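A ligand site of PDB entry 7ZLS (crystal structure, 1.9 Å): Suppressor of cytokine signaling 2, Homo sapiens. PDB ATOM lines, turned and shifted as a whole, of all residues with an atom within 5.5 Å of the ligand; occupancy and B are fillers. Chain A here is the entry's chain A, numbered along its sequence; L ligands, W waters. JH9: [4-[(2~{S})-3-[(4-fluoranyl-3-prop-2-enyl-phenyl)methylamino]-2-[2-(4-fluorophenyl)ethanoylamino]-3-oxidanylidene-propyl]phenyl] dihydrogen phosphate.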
ATOM      1  N   VAL A  26     -21.845 -20.696 -21.453  1.00  0.00           N
ATOM      2  CA  VAL A  26     -21.830 -21.807 -20.501  1.00  0.00           C
ATOM      3  C   VAL A  26     -22.418 -23.062 -21.131  1.00  0.00           C
ATOM      4  O   VAL A  26     -21.938 -24.180 -20.895  1.00  0.00           O
ATOM      5  CB  VAL A  26     -22.568 -21.418 -19.203  1.00  0.00           C
ATOM      6  CG1 VAL A  26     -24.037 -21.140 -19.457  1.00  0.00           C
ATOM      7  CG2 VAL A  26     -22.419 -22.518 -18.104  1.00  0.00           C
ATOM      8  N   ASN A  27     -23.455 -22.904 -21.964  1.00  0.00           N
ATOM      9  CA  ASN A  27     -24.075 -24.045 -22.628  1.00  0.00           C
ATOM     10  C   ASN A  27     -23.131 -24.652 -23.654  1.00  0.00           C
ATOM     11  O   ASN A  27     -23.004 -25.876 -23.745  1.00  0.00           O
ATOM     12  CB  ASN A  27     -25.369 -23.614 -23.312  1.00  0.00           C
ATOM     13  CG  ASN A  27     -26.313 -22.920 -22.364  1.00  0.00           C
ATOM     14  OD1 ASN A  27     -27.202 -23.559 -21.800  1.00  0.00           O
ATOM     15  ND2 ASN A  27     -26.088 -21.621 -22.150  1.00  0.00           N
ATOM     16  N   LYS A  30     -20.485 -26.556 -21.808  1.00  0.00           N
ATOM     17  CA  LYS A  30     -21.019 -27.840 -21.365  1.00  0.00           C
ATOM     18  C   LYS A  30     -21.005 -28.868 -22.494  1.00  0.00           C
ATOM     19  O   LYS A  30     -20.576 -30.022 -22.289  1.00  0.00           O
ATOM     20  CB  LYS A  30     -22.455 -27.669 -20.819  1.00  0.00           C
ATOM     21  CG  LYS A  30     -23.052 -28.953 -20.255  1.00  0.00           C
ATOM     22  CD  LYS A  30     -24.555 -28.886 -20.080  1.00  0.00           C
ATOM     23  CE  LYS A  30     -25.116 -30.218 -19.539  1.00  0.00           C
ATOM     24  NZ  LYS A  30     -26.610 -30.328 -19.531  1.00  0.00           N
ATOM     25  N   ARG A  44     -12.820 -19.234 -20.816  1.00  0.00           N
ATOM     26  CA  ARG A  44     -13.646 -18.469 -21.727  1.00  0.00           C
ATOM     27  C   ARG A  44     -14.081 -17.200 -21.014  1.00  0.00           C
ATOM     28  O   ARG A  44     -13.857 -17.036 -19.816  1.00  0.00           O
ATOM     29  CB  ARG A  44     -14.863 -19.294 -22.190  1.00  0.00           C
ATOM     30  CG  ARG A  44     -15.764 -19.695 -21.014  1.00  0.00           C
ATOM     31  CD  ARG A  44     -16.908 -20.647 -21.406  1.00  0.00           C
ATOM     32  NE  ARG A  44     -17.707 -21.059 -20.249  1.00  0.00           N
ATOM     33  CZ  ARG A  44     -18.549 -20.276 -19.587  1.00  0.00           C
ATOM     34  NH1 ARG A  44     -18.808 -19.031 -19.969  1.00  0.00           N
ATOM     35  NH2 ARG A  44     -19.151 -20.745 -18.504  1.00  0.00           N
ATOM     36  N   ASP A  45     -14.747 -16.313 -21.749  1.00  0.00           N
ATOM     37  CA  ASP A  45     -15.298 -15.112 -21.125  1.00  0.00           C
ATOM     38  C   ASP A  45     -16.475 -15.458 -20.232  1.00  0.00           C
ATOM     39  O   ASP A  45     -17.275 -16.341 -20.547  1.00  0.00           O
ATOM     40  CB  ASP A  45     -15.746 -14.130 -22.185  1.00  0.00           C
ATOM     41  CG  ASP A  45     -14.604 -13.608 -23.025  1.00  0.00           C
ATOM     42  OD1 ASP A  45     -13.412 -13.893 -22.718  1.00  0.00           O
ATOM     43  OD2 ASP A  45     -14.935 -12.907 -23.975  1.00  0.00           O
ATOM     44  N   SER A  46     -16.625 -14.699 -19.153  1.00  0.00           N
ATOM     45  CA  SER A  46     -17.752 -14.845 -18.235  1.00  0.00           C
ATOM     46  C   SER A  46     -18.949 -14.019 -18.687  1.00  0.00           C
ATOM     47  O   SER A  46     -18.801 -12.878 -19.142  1.00  0.00           O
ATOM     48  CB  SER A  46     -17.350 -14.401 -16.824  1.00  0.00           C
ATOM     49  OG  SER A  46     -18.470 -14.387 -15.946  1.00  0.00           O
ATOM     50  N   SER A  47     -20.152 -14.570 -18.513  1.00  0.00           N
ATOM     51  CA  SER A  47     -21.353 -13.768 -18.775  1.00  0.00           C
ATOM     52  C   SER A  47     -21.552 -12.645 -17.746  1.00  0.00           C
ATOM     53  O   SER A  47     -22.365 -11.745 -17.970  1.00  0.00           O
ATOM     54  CB  SER A  47     -22.594 -14.644 -18.765  1.00  0.00           C
ATOM     55  OG  SER A  47     -22.878 -15.064 -17.434  1.00  0.00           O
ATOM     56  N   HIS A  48     -20.866 -12.713 -16.605  1.00  0.00           N
ATOM     57  CA  HIS A  48     -21.152 -11.828 -15.475  1.00  0.00           C
ATOM     58  C   HIS A  48     -20.192 -10.645 -15.471  1.00  0.00           C
ATOM     59  O   HIS A  48     -18.968 -10.821 -15.581  1.00  0.00           O
ATOM     60  CB  HIS A  48     -21.045 -12.635 -14.175  1.00  0.00           C
ATOM     61  CG  HIS A  48     -21.705 -11.984 -12.994  1.00  0.00           C
ATOM     62  ND1 HIS A  48     -21.300 -10.769 -12.489  1.00  0.00           N
ATOM     63  CD2 HIS A  48     -22.741 -12.393 -12.232  1.00  0.00           C
ATOM     64  CE1 HIS A  48     -22.065 -10.458 -11.457  1.00  0.00           C
ATOM     65  NE2 HIS A  48     -22.945 -11.426 -11.283  1.00  0.00           N
ATOM     66  N   THR A  54     -14.003 -17.281 -16.961  1.00  0.00           N
ATOM     67  CA  THR A  54     -14.608 -18.442 -16.346  1.00  0.00           C
ATOM     68  C   THR A  54     -13.847 -19.693 -16.743  1.00  0.00           C
ATOM     69  O   THR A  54     -13.589 -19.908 -17.928  1.00  0.00           O
ATOM     70  CB  THR A  54     -16.069 -18.578 -16.781  1.00  0.00           C
ATOM     71  OG1 THR A  54     -16.836 -17.480 -16.267  1.00  0.00           O
ATOM     72  CG2 THR A  54     -16.659 -19.947 -16.307  1.00  0.00           C
ATOM     73  N   VAL A  57     -14.869 -26.911 -16.537  1.00  0.00           N
ATOM     74  CA  VAL A  57     -14.092 -28.133 -16.306  1.00  0.00           C
ATOM     75  C   VAL A  57     -15.042 -29.302 -16.145  1.00  0.00           C
ATOM     76  O   VAL A  57     -16.093 -29.188 -15.492  1.00  0.00           O
ATOM     77  CB  VAL A  57     -13.167 -27.973 -15.060  1.00  0.00           C
ATOM     78  CG1 VAL A  57     -13.961 -27.450 -13.872  1.00  0.00           C
ATOM     79  CG2 VAL A  57     -12.487 -29.295 -14.693  1.00  0.00           C
ATOM     80  N   PRO A  63     -19.981 -31.187 -16.640  1.00  0.00           N
ATOM     81  CA  PRO A  63     -19.228 -29.931 -16.695  1.00  0.00           C
ATOM     82  C   PRO A  63     -19.667 -28.952 -15.624  1.00  0.00           C
ATOM     83  O   PRO A  63     -20.849 -28.838 -15.290  1.00  0.00           O
ATOM     84  CB  PRO A  63     -19.513 -29.410 -18.113  1.00  0.00           C
ATOM     85  CG  PRO A  63     -19.818 -30.640 -18.916  1.00  0.00           C
ATOM     86  CD  PRO A  63     -20.620 -31.516 -17.934  1.00  0.00           C
ATOM     87  N   THR A  64     -18.689 -28.248 -15.059  1.00  0.00           N
ATOM     88  CA  THR A  64     -18.974 -27.217 -14.075  1.00  0.00           C
ATOM     89  C   THR A  64     -18.151 -25.988 -14.411  1.00  0.00           C
ATOM     90  O   THR A  64     -17.334 -25.994 -15.341  1.00  0.00           O
ATOM     91  CB  THR A  64     -18.719 -27.705 -12.625  1.00  0.00           C
ATOM     92  OG1 THR A  64     -19.389 -26.818 -11.718  1.00  0.00           O
ATOM     93  CG2 THR A  64     -17.238 -27.682 -12.314  1.00  0.00           C
ATOM     94  N   ASN A  65     -18.398 -24.891 -13.693  1.00  0.00           N
ATOM     95  CA  ASN A  65     -17.833 -23.601 -14.059  1.00  0.00           C
ATOM     96  C   ASN A  65     -17.412 -22.847 -12.812  1.00  0.00           C
ATOM     97  O   ASN A  65     -18.079 -22.909 -11.779  1.00  0.00           O
ATOM     98  CB  ASN A  65     -18.829 -22.749 -14.842  1.00  0.00           C
ATOM     99  CG  ASN A  65     -19.394 -23.493 -16.025  1.00  0.00           C
ATOM    100  OD1 ASN A  65     -18.894 -23.333 -17.144  1.00  0.00           O
ATOM    101  ND2 ASN A  65     -20.418 -24.339 -15.779  1.00  0.00           N
ATOM    102  N   LEU A  66     -16.309 -22.099 -12.940  1.00  0.00           N
ATOM    103  CA  LEU A  66     -15.709 -21.396 -11.810  1.00  0.00           C
ATOM    104  C   LEU A  66     -15.184 -20.066 -12.313  1.00  0.00           C
ATOM    105  O   LEU A  66     -14.346 -20.034 -13.210  1.00  0.00           O
ATOM    106  CB  LEU A  66     -14.591 -22.217 -11.172  1.00  0.00           C
ATOM    107  CG  LEU A  66     -13.925 -21.586  -9.955  1.00  0.00           C
ATOM    108  CD1 LEU A  66     -15.011 -21.157  -8.942  1.00  0.00           C
ATOM    109  CD2 LEU A  66     -12.875 -22.503  -9.319  1.00  0.00           C
ATOM    110  N   ARG A  67     -15.683 -18.973 -11.761  1.00  0.00           N
ATOM    111  CA  ARG A  67     -15.298 -17.672 -12.292  1.00  0.00           C
ATOM    112  C   ARG A  67     -13.959 -17.204 -11.707  1.00  0.00           C
ATOM    113  O   ARG A  67     -13.541 -17.633 -10.631  1.00  0.00           O
ATOM    114  CB  ARG A  67     -16.373 -16.634 -11.988  1.00  0.00           C
ATOM    115  CG  ARG A  67     -17.625 -16.851 -12.798  1.00  0.00           C
ATOM    116  CD  ARG A  67     -18.783 -16.064 -12.251  1.00  0.00           C
ATOM    117  NE  ARG A  67     -19.965 -16.261 -13.089  1.00  0.00           N
ATOM    118  CZ  ARG A  67     -21.207 -16.052 -12.699  1.00  0.00           C
ATOM    119  NH1 ARG A  67     -21.489 -15.663 -11.451  1.00  0.00           N
ATOM    120  NH2 ARG A  67     -22.192 -16.201 -13.575  1.00  0.00           N
ATOM    121  N   LEU A  77      -9.437 -16.807  -7.964  1.00  0.00           N
ATOM    122  CA  LEU A  77     -10.710 -17.511  -8.055  1.00  0.00           C
ATOM    123  C   LEU A  77     -11.798 -16.751  -7.325  1.00  0.00           C
ATOM    124  O   LEU A  77     -11.541 -16.015  -6.367  1.00  0.00           O
ATOM    125  CB  LEU A  77     -10.571 -18.914  -7.476  1.00  0.00           C
ATOM    126  CG  LEU A  77      -9.570 -19.838  -8.166  1.00  0.00           C
ATOM    127  CD1 LEU A  77      -9.536 -21.183  -7.463  1.00  0.00           C
ATOM    128  CD2 LEU A  77      -9.889 -19.976  -9.662  1.00  0.00           C
ATOM    129  N   ILE A  81     -17.522 -17.608  -3.531  1.00  0.00           N
ATOM    130  CA  ILE A  81     -17.619 -18.989  -3.085  1.00  0.00           C
ATOM    131  C   ILE A  81     -16.341 -19.482  -2.436  1.00  0.00           C
ATOM    132  O   ILE A  81     -16.401 -20.445  -1.641  1.00  0.00           O
ATOM    133  CB  ILE A  81     -18.042 -19.943  -4.236  1.00  0.00           C
ATOM    134  CG1 ILE A  81     -17.135 -19.797  -5.441  1.00  0.00           C
ATOM    135  CG2 ILE A  81     -19.462 -19.682  -4.657  1.00  0.00           C
ATOM    136  CD1 ILE A  81     -16.206 -20.956  -5.593  1.00  0.00           C
ATOM    137  N   CYS A  82     -15.209 -18.850  -2.678  1.00  0.00           N
ATOM    138  CA  CYS A  82     -13.964 -19.212  -2.014  1.00  0.00           C
ATOM    139  C   CYS A  82     -13.744 -18.318  -0.801  1.00  0.00           C
ATOM    140  O   CYS A  82     -14.193 -17.168  -0.769  1.00  0.00           O
ATOM    141  CB  CYS A  82     -12.795 -19.103  -2.979  1.00  0.00           C
ATOM    142  SG  CYS A  82     -12.995 -20.105  -4.477  1.00  0.00           S
ATOM    143  N   VAL A 119     -17.899 -28.639  -3.978  1.00  0.00           N
ATOM    144  CA  VAL A 119     -17.233 -28.937  -5.241  1.00  0.00           C
ATOM    145  C   VAL A 119     -15.760 -28.566  -5.181  1.00  0.00           C
ATOM    146  O   VAL A 119     -15.426 -27.406  -4.918  1.00  0.00           O
ATOM    147  CB  VAL A 119     -17.919 -28.199  -6.414  1.00  0.00           C
ATOM    148  N   HIS A 120     -14.873 -29.527  -5.424  1.00  0.00           N
ATOM    149  CA  HIS A 120     -13.436 -29.287  -5.423  1.00  0.00           C
ATOM    150  C   HIS A 120     -12.937 -29.020  -6.839  1.00  0.00           C
ATOM    151  O   HIS A 120     -13.486 -29.536  -7.821  1.00  0.00           O
ATOM    152  CB  HIS A 120     -12.668 -30.470  -4.825  1.00  0.00           C
ATOM    153  N   LEU A 121     -11.890 -28.187  -6.930  1.00  0.00           N
ATOM    154  CA  LEU A 121     -11.269 -27.853  -8.198  1.00  0.00           C
ATOM    155  C   LEU A 121     -10.259 -28.916  -8.589  1.00  0.00           C
ATOM    156  O   LEU A 121      -9.258 -29.131  -7.876  1.00  0.00           O
ATOM    157  CB  LEU A 121     -10.585 -26.482  -8.118  1.00  0.00           C
ATOM    158  CG  LEU A 121     -10.011 -25.992  -9.443  1.00  0.00           C
ATOM    159  CD1 LEU A 121     -11.111 -25.825 -10.516  1.00  0.00           C
ATOM    160  CD2 LEU A 121      -9.289 -24.676  -9.209  1.00  0.00           C
ATOM    161  N   TYR A 122     -10.488 -29.582  -9.716  1.00  0.00           N
ATOM    162  CA  TYR A 122      -9.581 -30.628 -10.183  1.00  0.00           C
ATOM    163  C   TYR A 122      -9.370 -30.411 -11.676  1.00  0.00           C
ATOM    164  O   TYR A 122     -10.296 -30.577 -12.471  1.00  0.00           O
ATOM    165  CB  TYR A 122     -10.146 -32.016  -9.882  1.00  0.00           C
ATOM    166  CG  TYR A 122      -9.272 -33.112 -10.415  1.00  0.00           C
ATOM    167  CD1 TYR A 122      -8.027 -33.380  -9.858  1.00  0.00           C
ATOM    168  CD2 TYR A 122      -9.692 -33.887 -11.509  1.00  0.00           C
ATOM    169  CE1 TYR A 122      -7.216 -34.395 -10.359  1.00  0.00           C
ATOM    170  CE2 TYR A 122      -8.897 -34.897 -12.012  1.00  0.00           C
ATOM    171  CZ  TYR A 122      -7.665 -35.160 -11.440  1.00  0.00           C
ATOM    172  OH  TYR A 122      -6.877 -36.161 -11.965  1.00  0.00           O
HETATM  173  C10 JH9 L   1     -24.474 -24.421 -14.931  1.00  0.00           C
HETATM  174  C13 JH9 L   1     -20.853 -23.018  -9.536  1.00  0.00           C
HETATM  175  C15 JH9 L   1     -19.092 -23.800  -7.943  1.00  0.00           C
HETATM  176  C17 JH9 L   1     -17.334 -25.187  -9.124  1.00  0.00           C
HETATM  177  C21 JH9 L   1     -15.569 -24.749  -7.026  1.00  0.00           C
HETATM  178  C22 JH9 L   1     -14.584 -24.543  -5.862  1.00  0.00           C
HETATM  179  C24 JH9 L   1     -12.598 -23.315  -5.106  1.00  0.00           C
HETATM  180  C28 JH9 L   1     -21.363 -20.696 -12.487  1.00  0.00           C
HETATM  181  C02 JH9 L   1     -22.281 -24.384 -12.512  1.00  0.00           C
HETATM  182  C03 JH9 L   1     -23.495 -25.266 -12.783  1.00  0.00           C
HETATM  183  C04 JH9 L   1     -23.713 -25.377 -14.271  1.00  0.00           C
HETATM  184  C05 JH9 L   1     -23.136 -26.424 -14.957  1.00  0.00           C
HETATM  185  C06 JH9 L   1     -23.314 -26.539 -16.330  1.00  0.00           C
HETATM  186  C07 JH9 L   1     -24.085 -25.594 -16.983  1.00  0.00           C
HETATM  187  C09 JH9 L   1     -24.674 -24.528 -16.299  1.00  0.00           C
HETATM  188  C12 JH9 L   1     -21.210 -22.690 -10.971  1.00  0.00           C
HETATM  189  C16 JH9 L   1     -17.705 -24.423  -8.029  1.00  0.00           C
HETATM  190  C18 JH9 L   1     -16.066 -25.733  -9.172  1.00  0.00           C
HETATM  191  C19 JH9 L   1     -15.192 -25.508  -8.117  1.00  0.00           C
HETATM  192  C23 JH9 L   1     -13.605 -23.368  -5.947  1.00  0.00           C
HETATM  193  C25 JH9 L   1     -16.828 -24.213  -6.982  1.00  0.00           C
HETATM  194  C27 JH9 L   1     -21.652 -21.239 -11.072  1.00  0.00           C
HETATM  195  C29 JH9 L   1     -20.204 -19.969 -12.747  1.00  0.00           C
HETATM  196  C30 JH9 L   1     -19.937 -19.491 -14.030  1.00  0.00           C
HETATM  197  C31 JH9 L   1     -20.844 -19.750 -15.061  1.00  0.00           C
HETATM  198  C37 JH9 L   1     -22.002 -20.477 -14.801  1.00  0.00           C
HETATM  199  C38 JH9 L   1     -22.247 -20.963 -13.524  1.00  0.00           C
HETATM  200  F08 JH9 L   1     -24.264 -25.700 -18.320  1.00  0.00           F
HETATM  201  F20 JH9 L   1     -13.952 -26.051  -8.122  1.00  0.00           F
HETATM  202  N11 JH9 L   1     -22.308 -23.559 -11.310  1.00  0.00           N
HETATM  203  N14 JH9 L   1     -19.498 -23.461  -9.289  1.00  0.00           N
HETATM  204  O01 JH9 L   1     -21.345 -24.373 -13.256  1.00  0.00           O
HETATM  205  O26 JH9 L   1     -21.650 -22.945  -8.648  1.00  0.00           O
HETATM  206  O32 JH9 L   1     -20.613 -19.297 -16.367  1.00  0.00           O
HETATM  207  O34 JH9 L   1     -20.511 -17.532 -18.164  1.00  0.00           O
HETATM  208  O35 JH9 L   1     -19.442 -17.038 -15.939  1.00  0.00           O
HETATM  209  O36 JH9 L   1     -21.899 -17.055 -16.167  1.00  0.00           O
HETATM  210  P33 JH9 L   1     -20.602 -17.663 -16.676  1.00  0.00           P
HETATM  211  O   HOH W   1     -23.254 -18.372 -10.303  1.00  0.00           O
HETATM  212  O   HOH W   2     -22.345 -24.825  -6.165  1.00  0.00           O
HETATM  213  O   HOH W   3      -9.769 -22.816  -3.993  1.00  0.00           O
HETATM  214  O   HOH W   4     -22.132 -18.086 -19.965  1.00  0.00           O
HETATM  215  O   HOH W   5     -24.334 -18.205 -16.598  1.00  0.00           O
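An oxygen (O36) of the ligand is in salt-bridge range of the guanidinium group (NH2) of Arg 67 (2.7 Å).
OG1 of Thr 64 sits at hydrogen-bond distance from O01 of the ligand (3.5 Å).
An oxygen (O34) of the ligand is in salt-bridge range of the guanidinium group of Arg 44.
The side-chain hydroxyl (OG) of Ser 47 sits at hydrogen-bond distance from an oxygen (O36) of the ligand, 2.6 Å away.
The backbone NH (N) of Asn 65 lies within hydrogen-bond range of an oxygen (O01) of the ligand (3.0 Å).
The side-chain hydroxyl of Ser 46 sits at hydrogen-bond distance from an oxygen (O35) of the ligand (2.8 Å).
OG1 of Thr 54 lies within hydrogen-bond range of O35 of the ligand (2.7 Å).
An oxygen (O34) of the ligand sits at hydrogen-bond distance from the backbone NH of Ser 47, at 3.0 Å.
O of Asn 65 lies within hydrogen-bond range of N14 of the ligand.
An oxygen (O01) of the ligand lies within hydrogen-bond range of the side-chain amide nitrogen (ND2) of Asn 65 (2.7 Å).
The backbone NH of Thr 54 is in hydrogen-bond range of the backbone carbonyl oxygen of Arg 44, at 2.9 Å.
The backbone carbonyl oxygen of Val 57 lies within hydrogen-bond range of the backbone NH of Thr 64 (2.8 Å).
NH2 of Arg 44 sits at hydrogen-bond distance from OD1 of Asn 65 (2.9 Å).
The backbone NH (N) of His 48 is in hydrogen-bond range of the side-chain hydroxyl (OG) of Ser 46 (3.0 Å).
F20 of the ligand sits close to N of Leu 121 (3.2 Å).
Residues that only touch the ligand: Val 119, Cys 82, Pro 63, His 120, Val 26, Leu 66, Ile 81 and Lys 30.
Water W4 lies within hydrogen-bond range of O34 of the ligand (2.5 Å), N of Val 26 (3.0 Å) and NH1 of Arg 44 (3.5 Å).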
